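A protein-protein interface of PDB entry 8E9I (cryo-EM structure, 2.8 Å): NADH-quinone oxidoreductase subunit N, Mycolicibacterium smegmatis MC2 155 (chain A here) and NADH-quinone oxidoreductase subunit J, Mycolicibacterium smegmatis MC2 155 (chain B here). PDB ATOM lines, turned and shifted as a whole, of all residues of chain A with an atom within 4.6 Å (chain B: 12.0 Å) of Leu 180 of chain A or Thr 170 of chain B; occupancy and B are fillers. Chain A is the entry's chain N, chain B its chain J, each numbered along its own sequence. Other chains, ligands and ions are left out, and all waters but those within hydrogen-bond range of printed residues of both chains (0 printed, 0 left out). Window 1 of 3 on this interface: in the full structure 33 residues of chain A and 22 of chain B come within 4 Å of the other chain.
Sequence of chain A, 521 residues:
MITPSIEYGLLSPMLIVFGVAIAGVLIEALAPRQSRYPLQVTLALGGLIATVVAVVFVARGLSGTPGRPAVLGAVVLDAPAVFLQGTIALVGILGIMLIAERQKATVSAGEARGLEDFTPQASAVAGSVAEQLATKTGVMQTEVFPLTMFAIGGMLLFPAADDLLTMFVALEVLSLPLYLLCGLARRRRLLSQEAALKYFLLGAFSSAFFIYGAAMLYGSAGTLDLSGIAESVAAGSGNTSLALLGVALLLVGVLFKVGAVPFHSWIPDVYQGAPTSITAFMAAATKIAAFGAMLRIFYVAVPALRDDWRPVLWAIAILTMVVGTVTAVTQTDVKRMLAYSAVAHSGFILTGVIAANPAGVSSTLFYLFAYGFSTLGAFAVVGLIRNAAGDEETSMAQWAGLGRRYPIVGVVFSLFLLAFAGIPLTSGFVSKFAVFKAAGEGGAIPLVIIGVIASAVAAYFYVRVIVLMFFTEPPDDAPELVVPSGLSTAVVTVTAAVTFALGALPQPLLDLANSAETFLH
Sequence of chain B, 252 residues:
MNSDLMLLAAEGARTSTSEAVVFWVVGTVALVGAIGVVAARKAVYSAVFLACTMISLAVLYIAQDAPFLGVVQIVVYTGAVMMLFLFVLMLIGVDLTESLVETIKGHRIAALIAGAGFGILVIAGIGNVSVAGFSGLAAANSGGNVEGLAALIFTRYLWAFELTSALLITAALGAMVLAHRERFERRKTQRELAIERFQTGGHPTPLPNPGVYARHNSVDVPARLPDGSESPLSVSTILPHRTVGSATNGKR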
ATOM      1  N   LEU A 147      -8.911   4.174  19.078  1.00  0.00           N
ATOM      2  CA  LEU A 147      -7.626   4.750  19.457  1.00  0.00           C
ATOM      3  C   LEU A 147      -7.809   5.793  20.544  1.00  0.00           C
ATOM      4  O   LEU A 147      -7.201   5.704  21.617  1.00  0.00           O
ATOM      5  CB  LEU A 147      -6.946   5.373  18.242  1.00  0.00           C
ATOM      6  CG  LEU A 147      -6.268   4.419  17.266  1.00  0.00           C
ATOM      7  CD1 LEU A 147      -5.810   5.175  16.032  1.00  0.00           C
ATOM      8  CD2 LEU A 147      -5.102   3.720  17.929  1.00  0.00           C
ATOM      9  N   PHE A 150      -8.543   4.156  23.744  1.00  0.00           N
ATOM     10  CA  PHE A 150      -7.342   3.594  24.345  1.00  0.00           C
ATOM     11  C   PHE A 150      -6.552   4.675  25.061  1.00  0.00           C
ATOM     12  O   PHE A 150      -6.178   4.508  26.228  1.00  0.00           O
ATOM     13  CB  PHE A 150      -6.484   2.907  23.287  1.00  0.00           C
ATOM     14  CG  PHE A 150      -6.908   1.500  22.991  1.00  0.00           C
ATOM     15  CD1 PHE A 150      -6.787   0.516  23.950  1.00  0.00           C
ATOM     16  CD2 PHE A 150      -7.425   1.162  21.758  1.00  0.00           C
ATOM     17  CE1 PHE A 150      -7.177  -0.775  23.684  1.00  0.00           C
ATOM     18  CE2 PHE A 150      -7.816  -0.131  21.489  1.00  0.00           C
ATOM     19  CZ  PHE A 150      -7.692  -1.098  22.451  1.00  0.00           C
ATOM     20  N   LEU A 176       1.009   6.148  22.444  1.00  0.00           N
ATOM     21  CA  LEU A 176       0.926   5.589  21.096  1.00  0.00           C
ATOM     22  C   LEU A 176      -0.357   5.996  20.387  1.00  0.00           C
ATOM     23  O   LEU A 176      -0.289   6.413  19.216  1.00  0.00           O
ATOM     24  CB  LEU A 176       1.078   4.066  21.154  1.00  0.00           C
ATOM     25  CG  LEU A 176       2.430   3.532  21.637  1.00  0.00           C
ATOM     26  CD1 LEU A 176       2.506   2.029  21.451  1.00  0.00           C
ATOM     27  CD2 LEU A 176       3.583   4.208  20.933  1.00  0.00           C
ATOM     28  N   PRO A 177      -1.533   5.919  21.009  1.00  0.00           N
ATOM     29  CA  PRO A 177      -2.731   6.447  20.343  1.00  0.00           C
ATOM     30  C   PRO A 177      -2.578   7.893  19.924  1.00  0.00           C
ATOM     31  O   PRO A 177      -3.029   8.268  18.839  1.00  0.00           O
ATOM     32  CB  PRO A 177      -3.818   6.272  21.409  1.00  0.00           C
ATOM     33  CG  PRO A 177      -3.361   5.152  22.229  1.00  0.00           C
ATOM     34  CD  PRO A 177      -1.867   5.260  22.279  1.00  0.00           C
ATOM     35  N   LEU A 178      -1.947   8.723  20.751  1.00  0.00           N
ATOM     36  CA  LEU A 178      -1.813  10.127  20.387  1.00  0.00           C
ATOM     37  C   LEU A 178      -0.800  10.305  19.269  1.00  0.00           C
ATOM     38  O   LEU A 178      -1.001  11.128  18.369  1.00  0.00           O
ATOM     39  CB  LEU A 178      -1.430  10.952  21.608  1.00  0.00           C
ATOM     40  CG  LEU A 178      -2.470  10.873  22.725  1.00  0.00           C
ATOM     41  CD1 LEU A 178      -1.924  11.491  23.988  1.00  0.00           C
ATOM     42  CD2 LEU A 178      -3.775  11.532  22.317  1.00  0.00           C
ATOM     43  N   TYR A 179       0.293   9.539  19.302  1.00  0.00           N
ATOM     44  CA  TYR A 179       1.208   9.539  18.167  1.00  0.00           C
ATOM     45  C   TYR A 179       0.456   9.279  16.875  1.00  0.00           C
ATOM     46  O   TYR A 179       0.661   9.976  15.877  1.00  0.00           O
ATOM     47  CB  TYR A 179       2.290   8.477  18.339  1.00  0.00           C
ATOM     48  CG  TYR A 179       3.147   8.618  19.563  1.00  0.00           C
ATOM     49  CD1 TYR A 179       3.265   9.823  20.228  1.00  0.00           C
ATOM     50  CD2 TYR A 179       3.862   7.535  20.041  1.00  0.00           C
ATOM     51  CE1 TYR A 179       4.056   9.937  21.349  1.00  0.00           C
ATOM     52  CE2 TYR A 179       4.655   7.640  21.149  1.00  0.00           C
ATOM     53  CZ  TYR A 179       4.753   8.838  21.797  1.00  0.00           C
ATOM     54  OH  TYR A 179       5.550   8.915  22.911  1.00  0.00           O
ATOM     55  N   LEU A 180      -0.417   8.273  16.873  1.00  0.00           N
ATOM     56  CA  LEU A 180      -1.142   7.938  15.652  1.00  0.00           C
ATOM     57  C   LEU A 180      -2.137   9.028  15.284  1.00  0.00           C
ATOM     58  O   LEU A 180      -2.238   9.426  14.120  1.00  0.00           O
ATOM     59  CB  LEU A 180      -1.856   6.603  15.821  1.00  0.00           C
ATOM     60  CG  LEU A 180      -0.916   5.422  16.038  1.00  0.00           C
ATOM     61  CD1 LEU A 180      -1.701   4.202  16.484  1.00  0.00           C
ATOM     62  CD2 LEU A 180      -0.127   5.145  14.776  1.00  0.00           C
ATOM     63  N   LEU A 181      -2.877   9.529  16.272  1.00  0.00           N
ATOM     64  CA  LEU A 181      -3.923  10.503  15.999  1.00  0.00           C
ATOM     65  C   LEU A 181      -3.353  11.801  15.457  1.00  0.00           C
ATOM     66  O   LEU A 181      -3.983  12.446  14.614  1.00  0.00           O
ATOM     67  CB  LEU A 181      -4.718  10.772  17.274  1.00  0.00           C
ATOM     68  CG  LEU A 181      -5.552   9.592  17.764  1.00  0.00           C
ATOM     69  CD1 LEU A 181      -5.760   9.680  19.258  1.00  0.00           C
ATOM     70  CD2 LEU A 181      -6.880   9.550  17.040  1.00  0.00           C
ATOM     71  N   CYS A 182      -2.165  12.193  15.907  1.00  0.00           N
ATOM     72  CA  CYS A 182      -1.613  13.472  15.486  1.00  0.00           C
ATOM     73  C   CYS A 182      -1.393  13.550  13.982  1.00  0.00           C
ATOM     74  O   CYS A 182      -1.261  14.656  13.448  1.00  0.00           O
ATOM     75  CB  CYS A 182      -0.300  13.738  16.218  1.00  0.00           C
ATOM     76  SG  CYS A 182      -0.520  14.313  17.914  1.00  0.00           S
ATOM     77  N   GLY A 183      -1.349  12.419  13.287  1.00  0.00           N
ATOM     78  CA  GLY A 183      -1.073  12.405  11.866  1.00  0.00           C
ATOM     79  C   GLY A 183      -2.259  12.189  10.957  1.00  0.00           C
ATOM     80  O   GLY A 183      -2.066  11.812   9.798  1.00  0.00           O
ATOM     81  N   LEU A 184      -3.485  12.413  11.425  1.00  0.00           N
ATOM     82  CA  LEU A 184      -4.674  12.069  10.657  1.00  0.00           C
ATOM     83  C   LEU A 184      -5.490  13.288  10.243  1.00  0.00           C
ATOM     84  O   LEU A 184      -6.640  13.136   9.824  1.00  0.00           O
ATOM     85  CB  LEU A 184      -5.552  11.109  11.459  1.00  0.00           C
ATOM     86  CG  LEU A 184      -4.867   9.938  12.154  1.00  0.00           C
ATOM     87  CD1 LEU A 184      -5.874   9.187  13.000  1.00  0.00           C
ATOM     88  CD2 LEU A 184      -4.217   9.009  11.156  1.00  0.00           C
ATOM     89  N   ALA B 160      -0.401  -4.703  34.252  1.00  0.00           N
ATOM     90  CA  ALA B 160       0.489  -4.286  33.176  1.00  0.00           C
ATOM     91  C   ALA B 160       0.475  -5.299  32.040  1.00  0.00           C
ATOM     92  O   ALA B 160       0.518  -4.934  30.857  1.00  0.00           O
ATOM     93  CB  ALA B 160       1.904  -4.099  33.718  1.00  0.00           C
ATOM     94  N   PHE B 161       0.429  -6.584  32.383  1.00  0.00           N
ATOM     95  CA  PHE B 161       0.354  -7.622  31.367  1.00  0.00           C
ATOM     96  C   PHE B 161      -0.904  -7.461  30.528  1.00  0.00           C
ATOM     97  O   PHE B 161      -0.886  -7.656  29.309  1.00  0.00           O
ATOM     98  CB  PHE B 161       0.393  -8.996  32.031  1.00  0.00           C
ATOM     99  CG  PHE B 161      -0.126 -10.096  31.165  1.00  0.00           C
ATOM    100  CD1 PHE B 161       0.476 -10.384  29.959  1.00  0.00           C
ATOM    101  CD2 PHE B 161      -1.214 -10.844  31.559  1.00  0.00           C
ATOM    102  CE1 PHE B 161       0.000 -11.399  29.161  1.00  0.00           C
ATOM    103  CE2 PHE B 161      -1.691 -11.860  30.765  1.00  0.00           C
ATOM    104  CZ  PHE B 161      -1.082 -12.135  29.566  1.00  0.00           C
ATOM    105  N   GLU B 162      -2.016  -7.125  31.175  1.00  0.00           N
ATOM    106  CA  GLU B 162      -3.246  -6.890  30.432  1.00  0.00           C
ATOM    107  C   GLU B 162      -3.108  -5.682  29.518  1.00  0.00           C
ATOM    108  O   GLU B 162      -3.551  -5.712  28.364  1.00  0.00           O
ATOM    109  CB  GLU B 162      -4.411  -6.703  31.400  1.00  0.00           C
ATOM    110  N   LEU B 163      -2.486  -4.613  30.011  1.00  0.00           N
ATOM    111  CA  LEU B 163      -2.344  -3.402  29.209  1.00  0.00           C
ATOM    112  C   LEU B 163      -1.397  -3.584  28.031  1.00  0.00           C
ATOM    113  O   LEU B 163      -1.469  -2.821  27.056  1.00  0.00           O
ATOM    114  CB  LEU B 163      -1.860  -2.261  30.087  1.00  0.00           C
ATOM    115  CG  LEU B 163      -2.865  -1.901  31.172  1.00  0.00           C
ATOM    116  CD1 LEU B 163      -2.146  -1.381  32.396  1.00  0.00           C
ATOM    117  CD2 LEU B 163      -3.851  -0.881  30.635  1.00  0.00           C
ATOM    118  N   THR B 164      -0.489  -4.553  28.103  1.00  0.00           N
ATOM    119  CA  THR B 164       0.293  -4.866  26.915  1.00  0.00           C
ATOM    120  C   THR B 164      -0.617  -5.201  25.743  1.00  0.00           C
ATOM    121  O   THR B 164      -0.263  -4.943  24.587  1.00  0.00           O
ATOM    122  CB  THR B 164       1.244  -6.025  27.181  1.00  0.00           C
ATOM    123  OG1 THR B 164       0.496  -7.155  27.639  1.00  0.00           O
ATOM    124  CG2 THR B 164       2.286  -5.631  28.212  1.00  0.00           C
ATOM    125  N   SER B 165      -1.791  -5.769  26.014  1.00  0.00           N
ATOM    126  CA  SER B 165      -2.745  -6.016  24.942  1.00  0.00           C
ATOM    127  C   SER B 165      -3.219  -4.713  24.323  1.00  0.00           C
ATOM    128  O   SER B 165      -3.395  -4.632  23.103  1.00  0.00           O
ATOM    129  CB  SER B 165      -3.936  -6.811  25.467  1.00  0.00           C
ATOM    130  OG  SER B 165      -4.788  -5.990  26.244  1.00  0.00           O
ATOM    131  N   ALA B 166      -3.444  -3.688  25.141  1.00  0.00           N
ATOM    132  CA  ALA B 166      -3.805  -2.389  24.592  1.00  0.00           C
ATOM    133  C   ALA B 166      -2.687  -1.847  23.721  1.00  0.00           C
ATOM    134  O   ALA B 166      -2.940  -1.284  22.653  1.00  0.00           O
ATOM    135  CB  ALA B 166      -4.128  -1.411  25.720  1.00  0.00           C
ATOM    136  N   LEU B 167      -1.442  -2.002  24.169  1.00  0.00           N
ATOM    137  CA  LEU B 167      -0.313  -1.584  23.341  1.00  0.00           C
ATOM    138  C   LEU B 167      -0.336  -2.298  21.994  1.00  0.00           C
ATOM    139  O   LEU B 167      -0.184  -1.673  20.936  1.00  0.00           O
ATOM    140  CB  LEU B 167       1.007  -1.855  24.063  1.00  0.00           C
ATOM    141  CG  LEU B 167       1.311  -1.038  25.313  1.00  0.00           C
ATOM    142  CD1 LEU B 167       2.533  -1.589  26.013  1.00  0.00           C
ATOM    143  CD2 LEU B 167       1.522   0.411  24.945  1.00  0.00           C
ATOM    144  N   LEU B 168      -0.536  -3.614  22.015  1.00  0.00           N
ATOM    145  CA  LEU B 168      -0.567  -4.381  20.775  1.00  0.00           C
ATOM    146  C   LEU B 168      -1.680  -3.895  19.856  1.00  0.00           C
ATOM    147  O   LEU B 168      -1.476  -3.714  18.649  1.00  0.00           O
ATOM    148  CB  LEU B 168      -0.746  -5.863  21.090  1.00  0.00           C
ATOM    149  CG  LEU B 168      -1.242  -6.733  19.935  1.00  0.00           C
ATOM    150  CD1 LEU B 168      -0.267  -6.693  18.773  1.00  0.00           C
ATOM    151  CD2 LEU B 168      -1.459  -8.154  20.405  1.00  0.00           C
ATOM    152  N   ILE B 169      -2.873  -3.691  20.409  1.00  0.00           N
ATOM    153  CA  ILE B 169      -4.007  -3.293  19.582  1.00  0.00           C
ATOM    154  C   ILE B 169      -3.768  -1.914  18.992  1.00  0.00           C
ATOM    155  O   ILE B 169      -4.102  -1.652  17.834  1.00  0.00           O
ATOM    156  CB  ILE B 169      -5.310  -3.332  20.394  1.00  0.00           C
ATOM    157  CG1 ILE B 169      -5.819  -4.765  20.496  1.00  0.00           C
ATOM    158  CG2 ILE B 169      -6.354  -2.451  19.728  1.00  0.00           C
ATOM    159  CD1 ILE B 169      -6.967  -4.942  21.444  1.00  0.00           C
ATOM    160  N   THR B 170      -3.223  -0.998  19.792  1.00  0.00           N
ATOM    161  CA  THR B 170      -2.948   0.339  19.283  1.00  0.00           C
ATOM    162  C   THR B 170      -1.926   0.289  18.162  1.00  0.00           C
ATOM    163  O   THR B 170      -2.048   1.012  17.169  1.00  0.00           O
ATOM    164  CB  THR B 170      -2.460   1.248  20.406  1.00  0.00           C
ATOM    165  OG1 THR B 170      -1.387   0.610  21.109  1.00  0.00           O
ATOM    166  CG2 THR B 170      -3.585   1.553  21.373  1.00  0.00           C
ATOM    167  N   ALA B 171      -0.900  -0.551  18.303  1.00  0.00           N
ATOM    168  CA  ALA B 171       0.066  -0.699  17.223  1.00  0.00           C
ATOM    169  C   ALA B 171      -0.609  -1.220  15.963  1.00  0.00           C
ATOM    170  O   ALA B 171      -0.364  -0.722  14.859  1.00  0.00           O
ATOM    171  CB  ALA B 171       1.196  -1.631  17.650  1.00  0.00           C
ATOM    172  N   ALA B 172      -1.471  -2.224  16.111  1.00  0.00           N
ATOM    173  CA  ALA B 172      -2.164  -2.765  14.946  1.00  0.00           C
ATOM    174  C   ALA B 172      -3.043  -1.708  14.292  1.00  0.00           C
ATOM    175  O   ALA B 172      -3.087  -1.597  13.062  1.00  0.00           O
ATOM    176  CB  ALA B 172      -3.000  -3.978  15.349  1.00  0.00           C
ATOM    177  N   LEU B 173      -3.758  -0.929  15.101  1.00  0.00           N
ATOM    178  CA  LEU B 173      -4.642   0.094  14.558  1.00  0.00           C
ATOM    179  C   LEU B 173      -3.849   1.172  13.846  1.00  0.00           C
ATOM    180  O   LEU B 173      -4.258   1.656  12.788  1.00  0.00           O
ATOM    181  CB  LEU B 173      -5.479   0.708  15.674  1.00  0.00           C
ATOM    182  CG  LEU B 173      -6.548  -0.201  16.268  1.00  0.00           C
ATOM    183  CD1 LEU B 173      -6.964   0.331  17.618  1.00  0.00           C
ATOM    184  CD2 LEU B 173      -7.739  -0.315  15.339  1.00  0.00           C
ATOM    185  N   GLY B 174      -2.717   1.575  14.418  1.00  0.00           N
ATOM    186  CA  GLY B 174      -1.869   2.539  13.742  1.00  0.00           C
ATOM    187  C   GLY B 174      -1.357   2.014  12.419  1.00  0.00           C
ATOM    188  O   GLY B 174      -1.383   2.714  11.404  1.00  0.00           O
ATOM    189  N   ALA B 175      -0.894   0.767  12.409  1.00  0.00           N
ATOM    190  CA  ALA B 175      -0.419   0.180  11.167  1.00  0.00           C
ATOM    191  C   ALA B 175      -1.522   0.174  10.117  1.00  0.00           C
ATOM    192  O   ALA B 175      -1.310   0.584   8.972  1.00  0.00           O
ATOM    193  CB  ALA B 175       0.092  -1.235  11.424  1.00  0.00           C
ATOM    194  N   MET B 176      -2.721  -0.261  10.500  1.00  0.00           N
ATOM    195  CA  MET B 176      -3.810  -0.346   9.536  1.00  0.00           C
ATOM    196  C   MET B 176      -4.236   1.034   9.053  1.00  0.00           C
ATOM    197  O   MET B 176      -4.544   1.216   7.871  1.00  0.00           O
ATOM    198  CB  MET B 176      -4.997  -1.078  10.152  1.00  0.00           C
ATOM    199  CG  MET B 176      -4.838  -2.579  10.208  1.00  0.00           C
ATOM    200  SD  MET B 176      -4.685  -3.317   8.578  1.00  0.00           S
ATOM    201  CE  MET B 176      -6.403  -3.564   8.160  1.00  0.00           C
ATOM    202  N   VAL B 177      -4.277   2.015   9.949  1.00  0.00           N
ATOM    203  CA  VAL B 177      -4.800   3.323   9.579  1.00  0.00           C
ATOM    204  C   VAL B 177      -3.804   4.082   8.717  1.00  0.00           C
ATOM    205  O   VAL B 177      -4.183   4.714   7.727  1.00  0.00           O
ATOM    206  CB  VAL B 177      -5.175   4.113  10.844  1.00  0.00           C
ATOM    207  CG1 VAL B 177      -5.423   5.562  10.505  1.00  0.00           C
ATOM    208  CG2 VAL B 177      -6.396   3.505  11.496  1.00  0.00           C
ATOM    209  N   LEU B 178      -2.522   4.041   9.072  1.00  0.00           N
ATOM    210  CA  LEU B 178      -1.516   4.821   8.366  1.00  0.00           C
ATOM    211  C   LEU B 178      -0.844   4.062   7.236  1.00  0.00           C
ATOM    212  O   LEU B 178      -0.436   4.684   6.250  1.00  0.00           O
ATOM    213  CB  LEU B 178      -0.439   5.299   9.339  1.00  0.00           C
ATOM    214  CG  LEU B 178      -0.901   6.210  10.470  1.00  0.00           C
ATOM    215  CD1 LEU B 178       0.206   6.365  11.487  1.00  0.00           C
ATOM    216  CD2 LEU B 178      -1.315   7.557   9.924  1.00  0.00           C
ATOM    217  N   ALA B 179      -0.709   2.744   7.347  1.00  0.00           N
ATOM    218  CA  ALA B 179       0.012   1.971   6.347  1.00  0.00           C
ATOM    219  C   ALA B 179      -0.905   1.279   5.354  1.00  0.00           C
ATOM    220  O   ALA B 179      -0.727   1.443   4.145  1.00  0.00           O
ATOM    221  CB  ALA B 179       0.903   0.928   7.025  1.00  0.00           C
ATOM    222  N   HIS B 180      -1.878   0.505   5.821  1.00  0.00           N
ATOM    223  CA  HIS B 180      -2.747  -0.202   4.896  1.00  0.00           C
ATOM    224  C   HIS B 180      -3.412   0.784   3.952  1.00  0.00           C
ATOM    225  O   HIS B 180      -3.909   1.831   4.371  1.00  0.00           O
ATOM    226  CB  HIS B 180      -3.816  -0.991   5.642  1.00  0.00           C
ATOM    227  CG  HIS B 180      -4.605  -1.901   4.759  1.00  0.00           C
ATOM    228  ND1 HIS B 180      -5.980  -1.865   4.692  1.00  0.00           N
ATOM    229  CD2 HIS B 180      -4.211  -2.863   3.893  1.00  0.00           C
ATOM    230  CE1 HIS B 180      -6.400  -2.769   3.823  1.00  0.00           C
ATOM    231  NE2 HIS B 180      -5.346  -3.389   3.326  1.00  0.00           N
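The backbone carbonyl oxygen (O) of Ala 166 of chain B sits at hydrogen-bond distance from the side-chain hydroxyl (OG1) of Thr 170 of chain B. The backbone carbonyl oxygen (O) of Leu 167 of chain B is in hydrogen-bond range of the side-chain hydroxyl (OG1) of Thr 170 of chain B (2.6 Å).
Among the printed residues, pairs that only touch across the chains: Leu 180 of chain A with Gly 174 of chain B (3.2 Å), Phe 150 of chain A with Ile 169 of chain B (3.3 Å), Leu 180 of chain A with Thr 170 of chain B (3.3 Å), Leu 184 of chain A with Leu 178 of chain B (3.5 Å), Leu 180 of chain A with Leu 178 of chain B (3.5 Å), Phe 150 of chain A with Thr 170 of chain B (3.7 Å), Pro 177 of chain A with Thr 170 of chain B (3.7 Å), Leu 184 of chain A with Val 177 of chain B (3.7 Å), Phe 150 of chain A with Ala 166 of chain B (3.7 Å), Leu 147 of chain A with Leu 173 of chain B (3.8 Å), Leu 176 of chain A with Leu 167 of chain B (3.97 Å) and Phe 150 of chain A with Leu 173 of chain B (3.99 Å).
No residue of chain B comes within 4 Å of Leu 181 of chain A. No residue of chain B comes within 4 Å of Cys 182 of chain A. No residue of chain B comes within 4 Å of Gly 183 of chain A. Leu 184 of chain A touches just these residues of chain B: Val 177 (3.7 Å) and Leu 178 (3.5 Å). Of the printed residues of chain A, Gly 174 of chain B touches Leu 180. Printed residues of chain A within 4 Å of Leu 178 of chain B: Leu 180 and Leu 184. Of the printed residues of chain A, Ala 166 of chain B touches Phe 150. Printed residues of chain A within 4 Å of Leu 167 of chain B: Leu 176 (3.97 Å). Of the printed residues of chain A, Val 177 of chain B touches Leu 184. The nearest residue of chain B that does not touch Leu 180 of chain A is Leu 173 of chain B (4.6 Å).
Hydrophobic or aromatic side chains of chain A within 4 Å of the printed part of chain B: Leu 147, Phe 150, Leu 176, Pro 177, Leu 180 and Leu 184. Along chain A the printed residues that touch a printed residue of chain B span positions 147 to 184. Of the 21 printed residues of chain B, 8 touch a printed residue of chain A. Along chain B the printed residues that touch a printed residue of chain A span positions 166 to 178. Among the printed residues, 12 pairs touch across the chains. Among the printed residues, no Asp or Glu carboxylate lies within 4 Å of a Lys or Arg side-chain nitrogen of the other chain.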
